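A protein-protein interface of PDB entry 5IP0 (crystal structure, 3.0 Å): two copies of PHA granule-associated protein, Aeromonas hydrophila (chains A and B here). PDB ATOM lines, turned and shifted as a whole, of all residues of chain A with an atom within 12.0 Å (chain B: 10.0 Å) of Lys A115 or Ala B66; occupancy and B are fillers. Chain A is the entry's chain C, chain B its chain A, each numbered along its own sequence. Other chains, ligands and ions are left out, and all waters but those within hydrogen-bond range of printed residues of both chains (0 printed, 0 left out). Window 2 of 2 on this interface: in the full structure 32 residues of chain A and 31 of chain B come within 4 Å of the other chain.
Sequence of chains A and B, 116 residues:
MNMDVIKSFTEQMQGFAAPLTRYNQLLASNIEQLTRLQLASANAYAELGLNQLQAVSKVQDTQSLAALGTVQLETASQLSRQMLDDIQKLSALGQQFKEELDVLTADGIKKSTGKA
The backbone carbonyl oxygen of Gly A108 lies close to the backbone carbonyl oxygen of Gly B69, at 3.2 Å. The side-chain amide nitrogen (NE2) of Gln B72 sits at hydrogen-bond distance from the side-chain carboxylate (OD2) of Asp A107 (3.0 Å). NE2 of Gln B72 sits at hydrogen-bond distance from O of Leu A104. NZ of Lys A111 is in hydrogen-bond range of OE1 of Gln B72 (2.5 Å).
Gly A108 touches Gln B72 (N to NE2, 3.7 Å). Gly A108 touches Leu B73. Ile A109 touches Leu B73. Leu B65 touches Lys A111. CA of Ala B66 touches O of Lys A111, 3.3 Å away. Gly B69 touches Lys A111. Ala B66 touches Ser A112. CB of Ser A112 touches N of Thr B70 (3.98 Å). CD1 of Leu B73 touches OG of Ser A112 (3.8 Å). Ala B66 touches Lys A115 (CB to N, 3.3 Å).
OD1 of Asp A107 lies within salt-bridge range of NZ of Lys A111 (3.7 Å). The backbone carbonyl oxygen of Ile A109 is in hydrogen-bond range of the side-chain hydroxyl of Ser A112 (2.7 Å).
Along chain B the printed residues that touch a printed residue of chain A span positions 65 to 73. Hydrophobic or aromatic side chains of chain A within 4 Å of the printed part of chain B: Ile A109. Among the printed residues, 14 pairs touch across the chains. Among the printed residues, no Asp or Glu carboxylate lies within 4 Å of a Lys or Arg side-chain nitrogen of the other chain.
No position is printed for both chains.
Lys A115 touches just one residue of chain B: Ala B66 (3.3 Å). Printed residues of chain A within 4 Å of Ala B66: Lys A111 (3.3 Å), Ser A112 (3.5 Å) and Lys A115 (3.3 Å). No residue of chain B comes within 4 Å of Gly A114. Leu B65 touches one residue of chain A. No residue of chain A comes within 4 Å of Ala B67. Of chain A, only Gly A108 and Lys A111 come within 4 Å of Gly B69. Printed residues of chain A within 4 Å of Thr B70: Ser A112 (3.98 Å). Printed residues of chain B within 4 Å of Asp A107: Gln B72 (3.0 Å). Of the printed residues of chain B, Leu A104 touches Gln B72. Ala A106 touches none of the printed residues of chain B. Glu B74 touches none of the printed residues of chain A.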
ATOM      1  N   LEU A 104      23.211  -0.260  14.508  1.00  0.00           N
ATOM      2  CA  LEU A 104      23.402  -1.558  13.872  1.00  0.00           C
ATOM      3  C   LEU A 104      22.121  -2.056  13.216  1.00  0.00           C
ATOM      4  O   LEU A 104      22.164  -2.570  12.088  1.00  0.00           O
ATOM      5  CB  LEU A 104      23.924  -2.579  14.888  1.00  0.00           C
ATOM      6  CG  LEU A 104      25.448  -2.643  15.115  1.00  0.00           C
ATOM      7  CD1 LEU A 104      25.805  -3.885  15.887  1.00  0.00           C
ATOM      8  CD2 LEU A 104      26.218  -2.598  13.811  1.00  0.00           C
ATOM      9  N   THR A 105      20.962  -1.895  13.878  1.00  0.00           N
ATOM     10  CA  THR A 105      19.735  -2.333  13.219  1.00  0.00           C
ATOM     11  C   THR A 105      19.368  -1.426  12.038  1.00  0.00           C
ATOM     12  O   THR A 105      18.819  -1.913  11.045  1.00  0.00           O
ATOM     13  CB  THR A 105      18.556  -2.469  14.213  1.00  0.00           C
ATOM     14  OG1 THR A 105      17.481  -1.616  13.819  1.00  0.00           O
ATOM     15  CG2 THR A 105      18.935  -2.197  15.653  1.00  0.00           C
ATOM     16  N   ALA A 106      19.695  -0.132  12.083  1.00  0.00           N
ATOM     17  CA  ALA A 106      19.361   0.699  10.927  1.00  0.00           C
ATOM     18  C   ALA A 106      20.260   0.408   9.729  1.00  0.00           C
ATOM     19  O   ALA A 106      19.818   0.531   8.574  1.00  0.00           O
ATOM     20  CB  ALA A 106      19.435   2.177  11.297  1.00  0.00           C
ATOM     21  N   ASP A 107      21.525   0.047   9.983  1.00  0.00           N
ATOM     22  CA  ASP A 107      22.389  -0.475   8.922  1.00  0.00           C
ATOM     23  C   ASP A 107      21.832  -1.784   8.363  1.00  0.00           C
ATOM     24  O   ASP A 107      21.858  -2.020   7.144  1.00  0.00           O
ATOM     25  CB  ASP A 107      23.810  -0.661   9.477  1.00  0.00           C
ATOM     26  CG  ASP A 107      24.829  -1.135   8.424  1.00  0.00           C
ATOM     27  OD1 ASP A 107      24.941  -0.512   7.338  1.00  0.00           O
ATOM     28  OD2 ASP A 107      25.543  -2.126   8.713  1.00  0.00           O
ATOM     29  N   GLY A 108      21.309  -2.643   9.246  1.00  0.00           N
ATOM     30  CA  GLY A 108      20.635  -3.847   8.783  1.00  0.00           C
ATOM     31  C   GLY A 108      19.449  -3.560   7.880  1.00  0.00           C
ATOM     32  O   GLY A 108      19.243  -4.246   6.876  1.00  0.00           O
ATOM     33  N   ILE A 109      18.661  -2.541   8.218  1.00  0.00           N
ATOM     34  CA  ILE A 109      17.518  -2.184   7.391  1.00  0.00           C
ATOM     35  C   ILE A 109      17.970  -1.675   6.023  1.00  0.00           C
ATOM     36  O   ILE A 109      17.419  -2.075   4.989  1.00  0.00           O
ATOM     37  CB  ILE A 109      16.641  -1.155   8.116  1.00  0.00           C
ATOM     38  CG1 ILE A 109      16.018  -1.762   9.371  1.00  0.00           C
ATOM     39  CG2 ILE A 109      15.565  -0.682   7.198  1.00  0.00           C
ATOM     40  CD1 ILE A 109      15.121  -0.794  10.122  1.00  0.00           C
ATOM     41  N   LYS A 110      18.965  -0.781   5.990  1.00  0.00           N
ATOM     42  CA  LYS A 110      19.434  -0.262   4.702  1.00  0.00           C
ATOM     43  C   LYS A 110      19.938  -1.389   3.790  1.00  0.00           C
ATOM     44  O   LYS A 110      19.613  -1.445   2.590  1.00  0.00           O
ATOM     45  CB  LYS A 110      20.518   0.793   4.944  1.00  0.00           C
ATOM     46  CG  LYS A 110      21.154   1.422   3.692  1.00  0.00           C
ATOM     47  CD  LYS A 110      22.333   2.335   4.089  1.00  0.00           C
ATOM     48  CE  LYS A 110      22.887   3.155   2.924  1.00  0.00           C
ATOM     49  NZ  LYS A 110      22.188   4.475   2.727  1.00  0.00           N
ATOM     50  N   LYS A 111      20.722  -2.318   4.351  1.00  0.00           N
ATOM     51  CA  LYS A 111      21.205  -3.447   3.555  1.00  0.00           C
ATOM     52  C   LYS A 111      20.055  -4.354   3.130  1.00  0.00           C
ATOM     53  O   LYS A 111      20.074  -4.929   2.032  1.00  0.00           O
ATOM     54  CB  LYS A 111      22.236  -4.242   4.344  1.00  0.00           C
ATOM     55  CG  LYS A 111      23.462  -3.479   4.819  1.00  0.00           C
ATOM     56  CD  LYS A 111      24.448  -4.466   5.469  1.00  0.00           C
ATOM     57  CE  LYS A 111      25.640  -3.776   6.096  1.00  0.00           C
ATOM     58  NZ  LYS A 111      25.720  -4.159   7.530  1.00  0.00           N
ATOM     59  N   SER A 112      19.046  -4.485   4.001  1.00  0.00           N
ATOM     60  CA  SER A 112      17.894  -5.340   3.740  1.00  0.00           C
ATOM     61  C   SER A 112      17.065  -4.827   2.574  1.00  0.00           C
ATOM     62  O   SER A 112      16.435  -5.619   1.859  1.00  0.00           O
ATOM     63  CB  SER A 112      17.018  -5.432   4.994  1.00  0.00           C
ATOM     64  OG  SER A 112      16.018  -4.425   5.016  1.00  0.00           O
ATOM     65  N   THR A 113      17.023  -3.512   2.382  1.00  0.00           N
ATOM     66  CA  THR A 113      16.449  -3.010   1.143  1.00  0.00           C
ATOM     67  C   THR A 113      17.412  -3.143  -0.019  1.00  0.00           C
ATOM     68  O   THR A 113      16.987  -3.001  -1.169  1.00  0.00           O
ATOM     69  CB  THR A 113      16.071  -1.549   1.267  1.00  0.00           C
ATOM     70  OG1 THR A 113      17.220  -0.766   0.929  1.00  0.00           O
ATOM     71  CG2 THR A 113      15.630  -1.238   2.689  1.00  0.00           C
ATOM     72  N   GLY A 114      18.700  -3.347   0.259  1.00  0.00           N
ATOM     73  CA  GLY A 114      19.667  -3.622  -0.796  1.00  0.00           C
ATOM     74  C   GLY A 114      19.209  -4.472  -1.976  1.00  0.00           C
ATOM     75  O   GLY A 114      18.937  -3.945  -3.059  1.00  0.00           O
ATOM     76  N   LYS A 115      19.137  -5.788  -1.805  1.00  0.00           N
ATOM     77  CA  LYS A 115      18.762  -6.642  -2.936  1.00  0.00           C
ATOM     78  C   LYS A 115      17.245  -6.680  -3.094  1.00  0.00           C
ATOM     79  O   LYS A 115      16.555  -5.710  -2.776  1.00  0.00           O
ATOM     80  CB  LYS A 115      19.332  -8.064  -2.770  1.00  0.00           C
ATOM     81  N   ALA B  55      21.906 -18.744  10.362  1.00  0.00           N
ATOM     82  CA  ALA B  55      21.477 -17.719   9.419  1.00  0.00           C
ATOM     83  C   ALA B  55      22.604 -17.312   8.483  1.00  0.00           C
ATOM     84  O   ALA B  55      22.448 -17.346   7.257  1.00  0.00           O
ATOM     85  CB  ALA B  55      20.967 -16.502  10.190  1.00  0.00           C
ATOM     86  N   VAL B  59      22.933 -17.694   4.394  1.00  0.00           N
ATOM     87  CA  VAL B  59      23.339 -16.609   3.503  1.00  0.00           C
ATOM     88  C   VAL B  59      24.601 -16.993   2.745  1.00  0.00           C
ATOM     89  O   VAL B  59      24.786 -16.591   1.594  1.00  0.00           O
ATOM     90  CB  VAL B  59      23.531 -15.294   4.281  1.00  0.00           C
ATOM     91  CG1 VAL B  59      24.013 -14.186   3.359  1.00  0.00           C
ATOM     92  CG2 VAL B  59      22.236 -14.884   4.952  1.00  0.00           C
ATOM     93  N   THR B  62      24.025 -18.537  -0.677  1.00  0.00           N
ATOM     94  CA  THR B  62      23.332 -17.613  -1.570  1.00  0.00           C
ATOM     95  C   THR B  62      24.193 -16.358  -1.626  1.00  0.00           C
ATOM     96  O   THR B  62      25.278 -16.327  -1.035  1.00  0.00           O
ATOM     97  CB  THR B  62      21.908 -17.281  -1.105  1.00  0.00           C
ATOM     98  OG1 THR B  62      21.326 -16.336  -2.009  1.00  0.00           O
ATOM     99  CG2 THR B  62      21.921 -16.673   0.273  1.00  0.00           C
ATOM    100  N   GLN B  63      23.749 -15.320  -2.323  1.00  0.00           N
ATOM    101  CA  GLN B  63      24.578 -14.134  -2.475  1.00  0.00           C
ATOM    102  C   GLN B  63      23.925 -12.850  -1.993  1.00  0.00           C
ATOM    103  O   GLN B  63      24.634 -11.853  -1.813  1.00  0.00           O
ATOM    104  CB  GLN B  63      24.998 -13.962  -3.944  1.00  0.00           C
ATOM    105  CG  GLN B  63      26.336 -14.614  -4.285  1.00  0.00           C
ATOM    106  CD  GLN B  63      26.409 -16.084  -3.882  1.00  0.00           C
ATOM    107  OE1 GLN B  63      27.238 -16.478  -3.052  1.00  0.00           O
ATOM    108  NE2 GLN B  63      25.543 -16.904  -4.475  1.00  0.00           N
ATOM    109  N   SER B  64      22.610 -12.851  -1.770  1.00  0.00           N
ATOM    110  CA  SER B  64      21.855 -11.643  -1.459  1.00  0.00           C
ATOM    111  C   SER B  64      22.390 -11.024  -0.182  1.00  0.00           C
ATOM    112  O   SER B  64      22.298 -11.629   0.893  1.00  0.00           O
ATOM    113  CB  SER B  64      20.376 -11.969  -1.297  1.00  0.00           C
ATOM    114  OG  SER B  64      20.164 -12.563  -0.027  1.00  0.00           O
ATOM    115  N   LEU B  65      22.949  -9.817  -0.297  1.00  0.00           N
ATOM    116  CA  LEU B  65      23.359  -9.070   0.884  1.00  0.00           C
ATOM    117  C   LEU B  65      22.161  -8.521   1.635  1.00  0.00           C
ATOM    118  O   LEU B  65      22.313  -8.086   2.788  1.00  0.00           O
ATOM    119  CB  LEU B  65      24.304  -7.945   0.484  1.00  0.00           C
ATOM    120  CG  LEU B  65      25.583  -8.455  -0.181  1.00  0.00           C
ATOM    121  CD1 LEU B  65      26.580  -7.340  -0.410  1.00  0.00           C
ATOM    122  CD2 LEU B  65      26.204  -9.577   0.648  1.00  0.00           C
ATOM    123  N   ALA B  66      20.989  -8.534   0.986  1.00  0.00           N
ATOM    124  CA  ALA B  66      19.734  -8.170   1.631  1.00  0.00           C
ATOM    125  C   ALA B  66      19.347  -9.168   2.717  1.00  0.00           C
ATOM    126  O   ALA B  66      18.896  -8.771   3.795  1.00  0.00           O
ATOM    127  CB  ALA B  66      18.634  -8.070   0.585  1.00  0.00           C
ATOM    128  N   ALA B  67      19.461 -10.472   2.436  1.00  0.00           N
ATOM    129  CA  ALA B  67      19.183 -11.467   3.468  1.00  0.00           C
ATOM    130  C   ALA B  67      20.149 -11.312   4.633  1.00  0.00           C
ATOM    131  O   ALA B  67      19.761 -11.448   5.802  1.00  0.00           O
ATOM    132  CB  ALA B  67      19.271 -12.876   2.882  1.00  0.00           C
ATOM    133  N   LEU B  68      21.413 -11.009   4.322  1.00  0.00           N
ATOM    134  CA  LEU B  68      22.399 -10.737   5.356  1.00  0.00           C
ATOM    135  C   LEU B  68      21.953  -9.553   6.203  1.00  0.00           C
ATOM    136  O   LEU B  68      21.963  -9.620   7.438  1.00  0.00           O
ATOM    137  CB  LEU B  68      23.769 -10.504   4.710  1.00  0.00           C
ATOM    138  CG  LEU B  68      25.046 -10.573   5.563  1.00  0.00           C
ATOM    139  CD1 LEU B  68      25.320  -9.270   6.297  1.00  0.00           C
ATOM    140  CD2 LEU B  68      24.932 -11.703   6.575  1.00  0.00           C
ATOM    141  N   GLY B  69      21.529  -8.467   5.547  1.00  0.00           N
ATOM    142  CA  GLY B  69      21.045  -7.317   6.284  1.00  0.00           C
ATOM    143  C   GLY B  69      19.808  -7.625   7.105  1.00  0.00           C
ATOM    144  O   GLY B  69      19.645  -7.110   8.211  1.00  0.00           O
ATOM    145  N   THR B  70      18.950  -8.512   6.612  1.00  0.00           N
ATOM    146  CA  THR B  70      17.742  -8.841   7.357  1.00  0.00           C
ATOM    147  C   THR B  70      18.094  -9.636   8.607  1.00  0.00           C
ATOM    148  O   THR B  70      17.457  -9.475   9.662  1.00  0.00           O
ATOM    149  CB  THR B  70      16.747  -9.577   6.449  1.00  0.00           C
ATOM    150  OG1 THR B  70      15.412  -9.200   6.799  1.00  0.00           O
ATOM    151  CG2 THR B  70      16.874 -11.087   6.523  1.00  0.00           C
ATOM    152  N   VAL B  71      19.100 -10.508   8.510  1.00  0.00           N
ATOM    153  CA  VAL B  71      19.552 -11.223   9.692  1.00  0.00           C
ATOM    154  C   VAL B  71      20.212 -10.250  10.673  1.00  0.00           C
ATOM    155  O   VAL B  71      19.971 -10.318  11.886  1.00  0.00           O
ATOM    156  CB  VAL B  71      20.496 -12.361   9.262  1.00  0.00           C
ATOM    157  CG1 VAL B  71      21.423 -12.782  10.390  1.00  0.00           C
ATOM    158  CG2 VAL B  71      19.692 -13.533   8.714  1.00  0.00           C
ATOM    159  N   GLN B  72      20.977  -9.274  10.160  1.00  0.00           N
ATOM    160  CA  GLN B  72      21.620  -8.287  11.027  1.00  0.00           C
ATOM    161  C   GLN B  72      20.571  -7.506  11.796  1.00  0.00           C
ATOM    162  O   GLN B  72      20.612  -7.406  13.029  1.00  0.00           O
ATOM    163  CB  GLN B  72      22.496  -7.354  10.183  1.00  0.00           C
ATOM    164  CG  GLN B  72      23.200  -6.231  10.937  1.00  0.00           C
ATOM    165  CD  GLN B  72      23.973  -5.295  10.015  1.00  0.00           C
ATOM    166  OE1 GLN B  72      24.168  -5.585   8.832  1.00  0.00           O
ATOM    167  NE2 GLN B  72      24.409  -4.161  10.552  1.00  0.00           N
ATOM    168  N   LEU B  73      19.572  -7.028  11.066  1.00  0.00           N
ATOM    169  CA  LEU B  73      18.451  -6.282  11.608  1.00  0.00           C
ATOM    170  C   LEU B  73      17.755  -7.062  12.717  1.00  0.00           C
ATOM    171  O   LEU B  73      17.586  -6.565  13.841  1.00  0.00           O
ATOM    172  CB  LEU B  73      17.500  -6.098  10.438  1.00  0.00           C
ATOM    173  CG  LEU B  73      16.242  -5.322  10.183  1.00  0.00           C
ATOM    174  CD1 LEU B  73      15.972  -5.490   8.686  1.00  0.00           C
ATOM    175  CD2 LEU B  73      15.126  -5.876  11.007  1.00  0.00           C
ATOM    176  N   GLU B  74      17.378  -8.315  12.424  1.00  0.00           N
ATOM    177  CA  GLU B  74      16.683  -9.150  13.402  1.00  0.00           C
ATOM    178  C   GLU B  74      17.504  -9.359  14.668  1.00  0.00           C
ATOM    179  O   GLU B  74      17.000  -9.206  15.787  1.00  0.00           O
ATOM    180  CB  GLU B  74      16.332 -10.500  12.775  1.00  0.00           C
ATOM    181  CG  GLU B  74      15.002 -10.538  12.017  1.00  0.00           C
ATOM    182  CD  GLU B  74      13.773 -10.809  12.897  1.00  0.00           C
ATOM    183  OE1 GLU B  74      13.879 -10.798  14.146  1.00  0.00           O
ATOM    184  OE2 GLU B  74      12.682 -11.025  12.321  1.00  0.00           O
